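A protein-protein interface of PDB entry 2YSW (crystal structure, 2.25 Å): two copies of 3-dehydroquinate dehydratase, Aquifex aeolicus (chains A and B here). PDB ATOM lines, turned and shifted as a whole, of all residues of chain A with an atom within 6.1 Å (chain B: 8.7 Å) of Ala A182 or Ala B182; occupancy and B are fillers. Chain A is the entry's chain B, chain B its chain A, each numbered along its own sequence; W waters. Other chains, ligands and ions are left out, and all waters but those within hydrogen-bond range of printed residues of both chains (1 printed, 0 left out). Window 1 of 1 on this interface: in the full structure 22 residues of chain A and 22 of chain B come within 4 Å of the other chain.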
ATOM      1  N   LEU A 157     -20.717   5.659  14.004  1.00  0.00           N
ATOM      2  CA  LEU A 157     -20.607   4.221  13.793  1.00  0.00           C
ATOM      3  C   LEU A 157     -19.296   3.821  13.108  1.00  0.00           C
ATOM      4  O   LEU A 157     -18.589   2.940  13.596  1.00  0.00           O
ATOM      5  CB  LEU A 157     -21.820   3.710  12.994  1.00  0.00           C
ATOM      6  CG  LEU A 157     -23.179   3.942  13.678  1.00  0.00           C
ATOM      7  CD1 LEU A 157     -24.329   3.508  12.781  1.00  0.00           C
ATOM      8  CD2 LEU A 157     -23.218   3.177  14.987  1.00  0.00           C
ATOM      9  N   LYS A 177     -31.709   7.637  15.809  1.00  0.00           N
ATOM     10  CA  LYS A 177     -32.547   6.510  16.201  1.00  0.00           C
ATOM     11  C   LYS A 177     -32.144   5.176  15.554  1.00  0.00           C
ATOM     12  O   LYS A 177     -32.207   4.124  16.197  1.00  0.00           O
ATOM     13  CB  LYS A 177     -34.010   6.833  15.893  1.00  0.00           C
ATOM     14  CG  LYS A 177     -35.012   5.872  16.492  1.00  0.00           C
ATOM     15  CD  LYS A 177     -36.425   6.371  16.225  1.00  0.00           C
ATOM     16  CE  LYS A 177     -37.469   5.417  16.782  1.00  0.00           C
ATOM     17  NZ  LYS A 177     -38.860   5.921  16.542  1.00  0.00           N
ATOM     18  N   ILE A 178     -31.721   5.212  14.292  1.00  0.00           N
ATOM     19  CA  ILE A 178     -31.306   3.986  13.610  1.00  0.00           C
ATOM     20  C   ILE A 178     -30.105   3.321  14.313  1.00  0.00           C
ATOM     21  O   ILE A 178     -29.937   2.101  14.242  1.00  0.00           O
ATOM     22  CB  ILE A 178     -30.969   4.269  12.105  1.00  0.00           C
ATOM     23  CG1 ILE A 178     -30.631   2.967  11.369  1.00  0.00           C
ATOM     24  CG2 ILE A 178     -29.792   5.226  11.996  1.00  0.00           C
ATOM     25  CD1 ILE A 178     -31.778   1.953  11.320  1.00  0.00           C
ATOM     26  N   SER A 179     -29.286   4.115  15.008  1.00  0.00           N
ATOM     27  CA  SER A 179     -28.114   3.582  15.710  1.00  0.00           C
ATOM     28  C   SER A 179     -28.484   2.594  16.813  1.00  0.00           C
ATOM     29  O   SER A 179     -27.701   1.706  17.145  1.00  0.00           O
ATOM     30  CB  SER A 179     -27.282   4.714  16.325  1.00  0.00           C
ATOM     31  OG  SER A 179     -27.934   5.272  17.449  1.00  0.00           O
ATOM     32  N   ARG A 180     -29.678   2.739  17.376  1.00  0.00           N
ATOM     33  CA  ARG A 180     -30.117   1.843  18.443  1.00  0.00           C
ATOM     34  C   ARG A 180     -30.354   0.435  17.906  1.00  0.00           C
ATOM     35  O   ARG A 180     -30.369  -0.539  18.665  1.00  0.00           O
ATOM     36  CB  ARG A 180     -31.386   2.388  19.095  1.00  0.00           C
ATOM     37  CG  ARG A 180     -31.173   3.728  19.784  1.00  0.00           C
ATOM     38  CD  ARG A 180     -32.478   4.292  20.329  1.00  0.00           C
ATOM     39  NE  ARG A 180     -32.300   5.616  20.923  1.00  0.00           N
ATOM     40  CZ  ARG A 180     -31.773   5.840  22.122  1.00  0.00           C
ATOM     41  NH1 ARG A 180     -31.361   4.827  22.880  1.00  0.00           N
ATOM     42  NH2 ARG A 180     -31.663   7.082  22.569  1.00  0.00           N
ATOM     43  N   LEU A 181     -30.530   0.334  16.592  1.00  0.00           N
ATOM     44  CA  LEU A 181     -30.746  -0.956  15.960  1.00  0.00           C
ATOM     45  C   LEU A 181     -29.493  -1.424  15.216  1.00  0.00           C
ATOM     46  O   LEU A 181     -29.060  -2.567  15.370  1.00  0.00           O
ATOM     47  CB  LEU A 181     -31.920  -0.880  14.971  1.00  0.00           C
ATOM     48  CG  LEU A 181     -32.213  -2.157  14.169  1.00  0.00           C
ATOM     49  CD1 LEU A 181     -32.601  -3.286  15.115  1.00  0.00           C
ATOM     50  CD2 LEU A 181     -33.335  -1.904  13.177  1.00  0.00           C
ATOM     51  N   ALA A 182     -28.910  -0.528  14.421  1.00  0.00           N
ATOM     52  CA  ALA A 182     -27.745  -0.854  13.605  1.00  0.00           C
ATOM     53  C   ALA A 182     -26.405  -0.914  14.332  1.00  0.00           C
ATOM     54  O   ALA A 182     -25.448  -1.510  13.829  1.00  0.00           O
ATOM     55  CB  ALA A 182     -27.650   0.126  12.442  1.00  0.00           C
ATOM     56  N   GLY A 183     -26.342  -0.289  15.504  1.00  0.00           N
ATOM     57  CA  GLY A 183     -25.111  -0.276  16.277  1.00  0.00           C
ATOM     58  C   GLY A 183     -24.521  -1.651  16.485  1.00  0.00           C
ATOM     59  O   GLY A 183     -23.305  -1.810  16.505  1.00  0.00           O
ATOM     60  N   TYR A 184     -25.382  -2.650  16.620  1.00  0.00           N
ATOM     61  CA  TYR A 184     -24.941  -4.021  16.833  1.00  0.00           C
ATOM     62  C   TYR A 184     -23.911  -4.525  15.813  1.00  0.00           C
ATOM     63  O   TYR A 184     -22.941  -5.184  16.184  1.00  0.00           O
ATOM     64  CB  TYR A 184     -26.155  -4.954  16.838  1.00  0.00           C
ATOM     65  CG  TYR A 184     -25.818  -6.421  16.999  1.00  0.00           C
ATOM     66  CD1 TYR A 184     -25.257  -6.907  18.185  1.00  0.00           C
ATOM     67  CD2 TYR A 184     -26.052  -7.323  15.965  1.00  0.00           C
ATOM     68  CE1 TYR A 184     -24.938  -8.259  18.332  1.00  0.00           C
ATOM     69  CE2 TYR A 184     -25.738  -8.674  16.100  1.00  0.00           C
ATOM     70  CZ  TYR A 184     -25.182  -9.136  17.282  1.00  0.00           C
ATOM     71  OH  TYR A 184     -24.865 -10.472  17.402  1.00  0.00           O
ATOM     72  N   VAL A 185     -24.105  -4.224  14.534  1.00  0.00           N
ATOM     73  CA  VAL A 185     -23.159  -4.702  13.531  1.00  0.00           C
ATOM     74  C   VAL A 185     -21.837  -3.945  13.607  1.00  0.00           C
ATOM     75  O   VAL A 185     -20.863  -4.319  12.965  1.00  0.00           O
ATOM     76  CB  VAL A 185     -23.747  -4.615  12.096  1.00  0.00           C
ATOM     77  CG1 VAL A 185     -25.112  -5.277  12.067  1.00  0.00           C
ATOM     78  CG2 VAL A 185     -23.821  -3.187  11.627  1.00  0.00           C
ATOM     79  N   PHE A 186     -21.812  -2.883  14.407  1.00  0.00           N
ATOM     80  CA  PHE A 186     -20.602  -2.097  14.595  1.00  0.00           C
ATOM     81  C   PHE A 186     -19.991  -2.403  15.955  1.00  0.00           C
ATOM     82  O   PHE A 186     -19.110  -1.689  16.420  1.00  0.00           O
ATOM     83  CB  PHE A 186     -20.903  -0.602  14.474  1.00  0.00           C
ATOM     84  CG  PHE A 186     -21.244  -0.167  13.069  1.00  0.00           C
ATOM     85  CD1 PHE A 186     -22.555  -0.243  12.604  1.00  0.00           C
ATOM     86  CD2 PHE A 186     -20.247   0.280  12.202  1.00  0.00           C
ATOM     87  CE1 PHE A 186     -22.872   0.116  11.296  1.00  0.00           C
ATOM     88  CE2 PHE A 186     -20.556   0.646  10.881  1.00  0.00           C
ATOM     89  CZ  PHE A 186     -21.869   0.562  10.430  1.00  0.00           C
ATOM     90  N   GLY A 187     -20.466  -3.463  16.598  1.00  0.00           N
ATOM     91  CA  GLY A 187     -19.911  -3.843  17.887  1.00  0.00           C
ATOM     92  C   GLY A 187     -20.653  -3.429  19.150  1.00  0.00           C
ATOM     93  O   GLY A 187     -20.196  -3.748  20.247  1.00  0.00           O
ATOM     94  N   TYR A 217     -31.569  -9.718  13.266  1.00  0.00           N
ATOM     95  CA  TYR A 217     -30.443 -10.478  13.782  1.00  0.00           C
ATOM     96  C   TYR A 217     -30.686 -11.933  14.219  1.00  0.00           C
ATOM     97  O   TYR A 217     -30.409 -12.292  15.369  1.00  0.00           O
ATOM     98  CB  TYR A 217     -29.797  -9.693  14.936  1.00  0.00           C
ATOM     99  CG  TYR A 217     -29.415  -8.272  14.567  1.00  0.00           C
ATOM    100  CD1 TYR A 217     -28.659  -8.009  13.425  1.00  0.00           C
ATOM    101  CD2 TYR A 217     -29.807  -7.191  15.356  1.00  0.00           C
ATOM    102  CE1 TYR A 217     -28.306  -6.706  13.075  1.00  0.00           C
ATOM    103  CE2 TYR A 217     -29.455  -5.883  15.016  1.00  0.00           C
ATOM    104  CZ  TYR A 217     -28.705  -5.650  13.872  1.00  0.00           C
ATOM    105  OH  TYR A 217     -28.329  -4.379  13.511  1.00  0.00           O
ATOM    106  N   MET B   1     -35.257   8.229   1.636  1.00  0.00           N
ATOM    107  CA  MET B   1     -35.082   6.790   1.211  1.00  0.00           C
ATOM    108  C   MET B   1     -36.225   6.347   0.267  1.00  0.00           C
ATOM    109  O   MET B   1     -37.393   6.224   0.687  1.00  0.00           O
ATOM    110  CB  MET B   1     -35.058   5.865   2.452  1.00  0.00           C
ATOM    111  CG  MET B   1     -34.968   4.360   2.144  1.00  0.00           C
ATOM    112  SD  MET B   1     -34.998   3.295   3.607  1.00  0.00           S
ATOM    113  CE  MET B   1     -33.441   2.867   3.636  1.00  0.00           C
ATOM    114  N   TYR B 150     -21.468  -9.909   9.960  1.00  0.00           N
ATOM    115  CA  TYR B 150     -21.943  -8.564  10.265  1.00  0.00           C
ATOM    116  C   TYR B 150     -20.835  -7.556   9.963  1.00  0.00           C
ATOM    117  O   TYR B 150     -21.105  -6.412   9.602  1.00  0.00           O
ATOM    118  CB  TYR B 150     -22.395  -8.465  11.734  1.00  0.00           C
ATOM    119  CG  TYR B 150     -23.720  -9.161  11.996  1.00  0.00           C
ATOM    120  CD1 TYR B 150     -24.853  -8.845  11.243  1.00  0.00           C
ATOM    121  CD2 TYR B 150     -23.836 -10.161  12.965  1.00  0.00           C
ATOM    122  CE1 TYR B 150     -26.066  -9.504  11.439  1.00  0.00           C
ATOM    123  CE2 TYR B 150     -25.055 -10.834  13.169  1.00  0.00           C
ATOM    124  CZ  TYR B 150     -26.160 -10.500  12.401  1.00  0.00           C
ATOM    125  OH  TYR B 150     -27.357 -11.168  12.574  1.00  0.00           O
ATOM    126  N   VAL B 153     -20.937  -6.173   6.552  1.00  0.00           N
ATOM    127  CA  VAL B 153     -21.930  -5.116   6.421  1.00  0.00           C
ATOM    128  C   VAL B 153     -21.313  -3.790   6.851  1.00  0.00           C
ATOM    129  O   VAL B 153     -21.362  -2.806   6.112  1.00  0.00           O
ATOM    130  CB  VAL B 153     -23.190  -5.416   7.287  1.00  0.00           C
ATOM    131  CG1 VAL B 153     -24.253  -4.374   7.035  1.00  0.00           C
ATOM    132  CG2 VAL B 153     -23.728  -6.800   6.955  1.00  0.00           C
ATOM    133  N   ALA B 154     -20.715  -3.778   8.040  1.00  0.00           N
ATOM    134  CA  ALA B 154     -20.081  -2.569   8.558  1.00  0.00           C
ATOM    135  C   ALA B 154     -18.994  -2.087   7.603  1.00  0.00           C
ATOM    136  O   ALA B 154     -18.847  -0.888   7.359  1.00  0.00           O
ATOM    137  CB  ALA B 154     -19.463  -2.835   9.939  1.00  0.00           C
ATOM    138  N   LEU B 157     -20.560  -0.468   4.260  1.00  0.00           N
ATOM    139  CA  LEU B 157     -21.123   0.844   4.554  1.00  0.00           C
ATOM    140  C   LEU B 157     -20.067   1.909   4.837  1.00  0.00           C
ATOM    141  O   LEU B 157     -20.140   3.010   4.288  1.00  0.00           O
ATOM    142  CB  LEU B 157     -22.106   0.751   5.724  1.00  0.00           C
ATOM    143  CG  LEU B 157     -23.328  -0.139   5.483  1.00  0.00           C
ATOM    144  CD1 LEU B 157     -24.092  -0.332   6.787  1.00  0.00           C
ATOM    145  CD2 LEU B 157     -24.220   0.487   4.407  1.00  0.00           C
ATOM    146  N   LEU B 169     -26.261   0.992  -1.851  1.00  0.00           N
ATOM    147  CA  LEU B 169     -25.506  -0.059  -1.165  1.00  0.00           C
ATOM    148  C   LEU B 169     -26.395  -1.167  -0.626  1.00  0.00           C
ATOM    149  O   LEU B 169     -27.337  -0.908   0.119  1.00  0.00           O
ATOM    150  CB  LEU B 169     -24.715   0.545   0.003  1.00  0.00           C
ATOM    151  CG  LEU B 169     -23.713   1.652  -0.344  1.00  0.00           C
ATOM    152  CD1 LEU B 169     -23.264   2.374   0.917  1.00  0.00           C
ATOM    153  CD2 LEU B 169     -22.529   1.049  -1.075  1.00  0.00           C
ATOM    154  N   GLY B 176     -26.763  -9.208   5.935  1.00  0.00           N
ATOM    155  CA  GLY B 176     -26.875  -7.841   5.450  1.00  0.00           C
ATOM    156  C   GLY B 176     -28.244  -7.191   5.450  1.00  0.00           C
ATOM    157  O   GLY B 176     -28.408  -6.059   4.980  1.00  0.00           O
ATOM    158  N   LYS B 177     -29.231  -7.894   5.982  1.00  0.00           N
ATOM    159  CA  LYS B 177     -30.594  -7.380   6.023  1.00  0.00           C
ATOM    160  C   LYS B 177     -30.656  -5.963   6.602  1.00  0.00           C
ATOM    161  O   LYS B 177     -31.353  -5.097   6.071  1.00  0.00           O
ATOM    162  CB  LYS B 177     -31.444  -8.345   6.841  1.00  0.00           C
ATOM    163  CG  LYS B 177     -32.946  -8.181   6.755  1.00  0.00           C
ATOM    164  CD  LYS B 177     -33.531  -9.525   7.183  1.00  0.00           C
ATOM    165  CE  LYS B 177     -35.002  -9.498   7.450  1.00  0.00           C
ATOM    166  NZ  LYS B 177     -35.445 -10.876   7.815  1.00  0.00           N
ATOM    167  N   ILE B 178     -29.912  -5.724   7.676  1.00  0.00           N
ATOM    168  CA  ILE B 178     -29.889  -4.413   8.318  1.00  0.00           C
ATOM    169  C   ILE B 178     -29.414  -3.312   7.358  1.00  0.00           C
ATOM    170  O   ILE B 178     -29.830  -2.158   7.479  1.00  0.00           O
ATOM    171  CB  ILE B 178     -28.984  -4.440   9.589  1.00  0.00           C
ATOM    172  CG1 ILE B 178     -29.022  -3.088  10.307  1.00  0.00           C
ATOM    173  CG2 ILE B 178     -27.551  -4.790   9.207  1.00  0.00           C
ATOM    174  CD1 ILE B 178     -30.385  -2.701  10.826  1.00  0.00           C
ATOM    175  N   SER B 179     -28.561  -3.665   6.395  1.00  0.00           N
ATOM    176  CA  SER B 179     -28.064  -2.679   5.437  1.00  0.00           C
ATOM    177  C   SER B 179     -29.208  -2.081   4.606  1.00  0.00           C
ATOM    178  O   SER B 179     -29.149  -0.919   4.196  1.00  0.00           O
ATOM    179  CB  SER B 179     -27.015  -3.307   4.492  1.00  0.00           C
ATOM    180  OG  SER B 179     -27.601  -4.092   3.452  1.00  0.00           O
ATOM    181  N   ARG B 180     -30.252  -2.869   4.369  1.00  0.00           N
ATOM    182  CA  ARG B 180     -31.386  -2.392   3.574  1.00  0.00           C
ATOM    183  C   ARG B 180     -32.140  -1.266   4.292  1.00  0.00           C
ATOM    184  O   ARG B 180     -32.857  -0.487   3.664  1.00  0.00           O
ATOM    185  CB  ARG B 180     -32.338  -3.550   3.262  1.00  0.00           C
ATOM    186  CG  ARG B 180     -31.673  -4.705   2.511  1.00  0.00           C
ATOM    187  CD  ARG B 180     -32.671  -5.815   2.195  1.00  0.00           C
ATOM    188  NE  ARG B 180     -32.045  -6.930   1.484  1.00  0.00           N
ATOM    189  CZ  ARG B 180     -31.925  -7.010   0.161  1.00  0.00           C
ATOM    190  NH1 ARG B 180     -32.397  -6.038  -0.620  1.00  0.00           N
ATOM    191  NH2 ARG B 180     -31.322  -8.061  -0.383  1.00  0.00           N
ATOM    192  N   LEU B 181     -31.970  -1.180   5.608  1.00  0.00           N
ATOM    193  CA  LEU B 181     -32.632  -0.134   6.379  1.00  0.00           C
ATOM    194  C   LEU B 181     -31.666   0.994   6.745  1.00  0.00           C
ATOM    195  O   LEU B 181     -31.967   2.171   6.535  1.00  0.00           O
ATOM    196  CB  LEU B 181     -33.249  -0.713   7.660  1.00  0.00           C
ATOM    197  CG  LEU B 181     -33.883   0.298   8.626  1.00  0.00           C
ATOM    198  CD1 LEU B 181     -35.054   1.003   7.938  1.00  0.00           C
ATOM    199  CD2 LEU B 181     -34.367  -0.419   9.887  1.00  0.00           C
ATOM    200  N   ALA B 182     -30.496   0.627   7.265  1.00  0.00           N
ATOM    201  CA  ALA B 182     -29.503   1.607   7.689  1.00  0.00           C
ATOM    202  C   ALA B 182     -28.666   2.233   6.582  1.00  0.00           C
ATOM    203  O   ALA B 182     -28.050   3.275   6.799  1.00  0.00           O
ATOM    204  CB  ALA B 182     -28.580   0.989   8.732  1.00  0.00           C
ATOM    205  N   GLY B 183     -28.634   1.610   5.407  1.00  0.00           N
ATOM    206  CA  GLY B 183     -27.832   2.149   4.320  1.00  0.00           C
ATOM    207  C   GLY B 183     -28.071   3.618   4.031  1.00  0.00           C
ATOM    208  O   GLY B 183     -27.166   4.350   3.619  1.00  0.00           O
ATOM    209  N   TYR B 184     -29.299   4.052   4.265  1.00  0.00           N
ATOM    210  CA  TYR B 184     -29.696   5.426   4.026  1.00  0.00           C
ATOM    211  C   TYR B 184     -28.806   6.471   4.715  1.00  0.00           C
ATOM    212  O   TYR B 184     -28.425   7.451   4.074  1.00  0.00           O
ATOM    213  CB  TYR B 184     -31.160   5.610   4.439  1.00  0.00           C
ATOM    214  CG  TYR B 184     -31.691   7.009   4.242  1.00  0.00           C
ATOM    215  CD1 TYR B 184     -31.767   7.576   2.970  1.00  0.00           C
ATOM    216  CD2 TYR B 184     -32.123   7.767   5.329  1.00  0.00           C
ATOM    217  CE1 TYR B 184     -32.257   8.863   2.786  1.00  0.00           C
ATOM    218  CE2 TYR B 184     -32.620   9.055   5.157  1.00  0.00           C
ATOM    219  CZ  TYR B 184     -32.683   9.598   3.886  1.00  0.00           C
ATOM    220  OH  TYR B 184     -33.158  10.877   3.721  1.00  0.00           O
ATOM    221  N   VAL B 185     -28.459   6.281   5.993  1.00  0.00           N
ATOM    222  CA  VAL B 185     -27.615   7.275   6.661  1.00  0.00           C
ATOM    223  C   VAL B 185     -26.183   7.295   6.131  1.00  0.00           C
ATOM    224  O   VAL B 185     -25.431   8.230   6.401  1.00  0.00           O
ATOM    225  CB  VAL B 185     -27.578   7.095   8.208  1.00  0.00           C
ATOM    226  CG1 VAL B 185     -29.006   7.053   8.760  1.00  0.00           C
ATOM    227  CG2 VAL B 185     -26.790   5.856   8.587  1.00  0.00           C
ATOM    228  N   PHE B 186     -25.813   6.269   5.369  1.00  0.00           N
ATOM    229  CA  PHE B 186     -24.476   6.193   4.790  1.00  0.00           C
ATOM    230  C   PHE B 186     -24.479   6.692   3.347  1.00  0.00           C
ATOM    231  O   PHE B 186     -23.462   6.625   2.667  1.00  0.00           O
ATOM    232  CB  PHE B 186     -23.957   4.756   4.838  1.00  0.00           C
ATOM    233  CG  PHE B 186     -23.735   4.245   6.229  1.00  0.00           C
ATOM    234  CD1 PHE B 186     -24.788   3.705   6.957  1.00  0.00           C
ATOM    235  CD2 PHE B 186     -22.485   4.337   6.824  1.00  0.00           C
ATOM    236  CE1 PHE B 186     -24.602   3.264   8.267  1.00  0.00           C
ATOM    237  CE2 PHE B 186     -22.283   3.900   8.133  1.00  0.00           C
ATOM    238  CZ  PHE B 186     -23.341   3.363   8.856  1.00  0.00           C
ATOM    239  N   GLY B 187     -25.619   7.188   2.880  1.00  0.00           N
ATOM    240  CA  GLY B 187     -25.685   7.700   1.521  1.00  0.00           C
ATOM    241  C   GLY B 187     -26.389   6.839   0.483  1.00  0.00           C
ATOM    242  O   GLY B 187     -26.382   7.190  -0.697  1.00  0.00           O
ATOM    243  N   SER B 188     -26.980   5.717   0.897  1.00  0.00           N
ATOM    244  CA  SER B 188     -27.691   4.853  -0.043  1.00  0.00           C
ATOM    245  C   SER B 188     -29.076   5.462  -0.270  1.00  0.00           C
ATOM    246  O   SER B 188     -29.892   5.540   0.653  1.00  0.00           O
ATOM    247  CB  SER B 188     -27.821   3.429   0.507  1.00  0.00           C
ATOM    248  OG  SER B 188     -28.432   2.592  -0.455  1.00  0.00           O
ATOM    249  N   THR B 191     -33.562   1.611  -1.668  1.00  0.00           N
ATOM    250  CA  THR B 191     -33.513   0.308  -1.017  1.00  0.00           C
ATOM    251  C   THR B 191     -34.501  -0.582  -1.765  1.00  0.00           C
ATOM    252  O   THR B 191     -35.448  -0.084  -2.376  1.00  0.00           O
ATOM    253  CB  THR B 191     -33.876   0.393   0.490  1.00  0.00           C
ATOM    254  OG1 THR B 191     -33.581  -0.862   1.115  1.00  0.00           O
ATOM    255  CG2 THR B 191     -35.358   0.715   0.686  1.00  0.00           C
ATOM    256  N   ILE B 204     -36.700  -7.791   2.920  1.00  0.00           N
ATOM    257  CA  ILE B 204     -37.699  -7.162   3.768  1.00  0.00           C
ATOM    258  C   ILE B 204     -38.945  -6.836   2.943  1.00  0.00           C
ATOM    259  O   ILE B 204     -38.849  -6.173   1.909  1.00  0.00           O
ATOM    260  CB  ILE B 204     -37.170  -5.837   4.368  1.00  0.00           C
ATOM    261  CG1 ILE B 204     -35.905  -6.096   5.188  1.00  0.00           C
ATOM    262  CG2 ILE B 204     -38.245  -5.192   5.234  1.00  0.00           C
ATOM    263  CD1 ILE B 204     -35.230  -4.828   5.678  1.00  0.00           C
ATOM    264  N   MET B 209     -40.938  -2.383   5.294  1.00  0.00           N
ATOM    265  CA  MET B 209     -39.964  -1.290   5.072  1.00  0.00           C
ATOM    266  C   MET B 209     -40.583   0.099   5.097  1.00  0.00           C
ATOM    267  O   MET B 209     -39.934   1.094   5.457  1.00  0.00           O
ATOM    268  CB  MET B 209     -39.240  -1.456   3.740  1.00  0.00           C
ATOM    269  CG  MET B 209     -38.158  -0.435   3.508  1.00  0.00           C
ATOM    270  SD  MET B 209     -36.749  -0.653   4.607  1.00  0.00           S
ATOM    271  CE  MET B 209     -35.980  -1.959   3.719  1.00  0.00           C
ATOM    272  N   LEU B 212     -41.008   0.891   8.690  1.00  0.00           N
ATOM    273  CA  LEU B 212     -39.670   1.157   9.214  1.00  0.00           C
ATOM    274  C   LEU B 212     -39.129   2.523   8.818  1.00  0.00           C
ATOM    275  O   LEU B 212     -38.483   3.198   9.616  1.00  0.00           O
ATOM    276  CB  LEU B 212     -38.696   0.072   8.749  1.00  0.00           C
ATOM    277  CG  LEU B 212     -38.930  -1.316   9.347  1.00  0.00           C
ATOM    278  CD1 LEU B 212     -38.079  -2.353   8.631  1.00  0.00           C
ATOM    279  CD2 LEU B 212     -38.607  -1.279  10.833  1.00  0.00           C
ATOM    280  N   PHE B 216     -37.971   5.245  11.671  1.00  0.00           N
ATOM    281  CA  PHE B 216     -36.587   5.666  11.840  1.00  0.00           C
ATOM    282  C   PHE B 216     -36.185   6.968  11.166  1.00  0.00           C
ATOM    283  O   PHE B 216     -35.305   7.665  11.646  1.00  0.00           O
ATOM    284  CB  PHE B 216     -35.652   4.545  11.361  1.00  0.00           C
ATOM    285  CG  PHE B 216     -35.618   3.357  12.280  1.00  0.00           C
ATOM    286  CD1 PHE B 216     -34.870   3.404  13.454  1.00  0.00           C
ATOM    287  CD2 PHE B 216     -36.337   2.199  11.986  1.00  0.00           C
ATOM    288  CE1 PHE B 216     -34.835   2.320  14.321  1.00  0.00           C
ATOM    289  CE2 PHE B 216     -36.307   1.106  12.854  1.00  0.00           C
ATOM    290  CZ  PHE B 216     -35.556   1.168  14.018  1.00  0.00           C
ATOM    291  N   TYR B 217     -36.816   7.308  10.054  1.00  0.00           N
ATOM    292  CA  TYR B 217     -36.417   8.521   9.350  1.00  0.00           C
ATOM    293  C   TYR B 217     -37.382   9.704   9.424  1.00  0.00           C
ATOM    294  O   TYR B 217     -38.542   9.624   9.023  1.00  0.00           O
ATOM    295  CB  TYR B 217     -36.037   8.143   7.908  1.00  0.00           C
ATOM    296  CG  TYR B 217     -34.887   7.146   7.910  1.00  0.00           C
ATOM    297  CD1 TYR B 217     -33.752   7.384   8.694  1.00  0.00           C
ATOM    298  CD2 TYR B 217     -34.942   5.955   7.177  1.00  0.00           C
ATOM    299  CE1 TYR B 217     -32.709   6.477   8.759  1.00  0.00           C
ATOM    300  CE2 TYR B 217     -33.893   5.027   7.230  1.00  0.00           C
ATOM    301  CZ  TYR B 217     -32.771   5.301   8.034  1.00  0.00           C
ATOM    302  OH  TYR B 217     -31.715   4.415   8.140  1.00  0.00           O
HETATM  303  O   HOH W   1     -32.578   7.222  12.480  1.00  0.00           O
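Water W1 lies within hydrogen-bond range of the backbone NH (N) of Ile A178, the backbone carbonyl oxygen (O) of Phe B216 and the backbone NH (N) of Lys A177.
O of Lys A177 touches CE1 of Phe B216, at 3.7 Å.
Ile A178 touches Ala B182.
CD1 of Phe B216 touches CA of Ile A178 (3.6 Å).
CD2 of Leu A181 touches CD2 of Leu B181 (3.8 Å).
CD2 of Leu A181 touches CZ of Phe B216 (3.9 Å).
CB of Ala A182 touches CB of Ala B182 (3.9 Å).
CG1 of Val A185 touches CD1 of Tyr B150, at 3.7 Å.
Ala B154 touches Phe A186 (CB to CE2, 3.8 Å).
Phe A186 touches Phe B186.
Tyr A217 touches Tyr B150.
Printed residues of chain A that touch a printed residue of chain B: Lys A177, Ile A178, Leu A181, Ala A182, Tyr A184, Val A185, Phe A186 and Tyr A217.
Hydrophobic or aromatic side chains of chain A within 4 Å of the printed part of chain B: Ile A178, Leu A181, Ala A182, Tyr A184, Val A185, Phe A186 and Tyr A217.
Of the 25 printed residues of chain B, 9 touch a printed residue of chain A.
Printed residues of chain B that touch a printed residue of chain A: Tyr B150, Ala B154, Ile B178, Leu B181, Ala B182, Val B185, Phe B186, Phe B216 and Tyr B217.
Hydrophobic or aromatic side chains of chain B that line the printed part of chain A: Tyr B150, Ala B154, Ile B178, Leu B181, Ala B182, Val B185, Phe B186, Phe B216 and Tyr B217.
Among the printed residues, 18 pairs touch across the chains.
Ile A178 touches Ala B182, but with the chains exchanged Ala A182 does not touch Ile B178 (4.1 Å).
Ile A178 touches Val B185, and with the chains exchanged Val A185 touches Ile B178.
Ile A178 touches Tyr B217, and with the chains exchanged Tyr A217 touches Ile B178.
Phe B186 touches its own counterpart, Phe A186.
13 positions are printed for both chains.
Of the 18 pairs that touch across the chains among the printed residues, 9 have their exchanged pair printed and touching as well.
Of the printed residues of chain B, Lys A177 touches Phe B216 (3.7 Å).
Ala A182 touches just one residue of chain B: Ala B182.
No residue of chain B comes within 4 Å of Gly A183.
Of the printed residues of chain B, Val A185 touches Tyr B150 (3.7 Å), Ala B154 (3.6 Å) and Ile B178 (3.8 Å).
Of the printed residues of chain A, Tyr B150 touches Tyr A184, Val A185 and Tyr A217.
Ser B179 touches none of the printed residues of chain A.
Of the printed residues of chain A, Leu B181 touches Ile A178 and Leu A181.
Ala B182 touches two residues of chain A.
Of the printed residues of chain A, Phe B186 touches Phe A186 (3.5 Å).
The nearest residue of chain B that does not touch Ala A182 is Ile B178 (4.1 Å).
The nearest printed residue of chain A that does not touch Ile B178 is Ala A182 (4.1 Å).
The backbone carbonyl oxygen of Leu B181 sits at hydrogen-bond distance from the side-chain hydroxyl of Tyr B217.
The backbone carbonyl oxygen (O) of Leu A181 sits at hydrogen-bond distance from the side-chain hydroxyl (OH) of Tyr A217.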
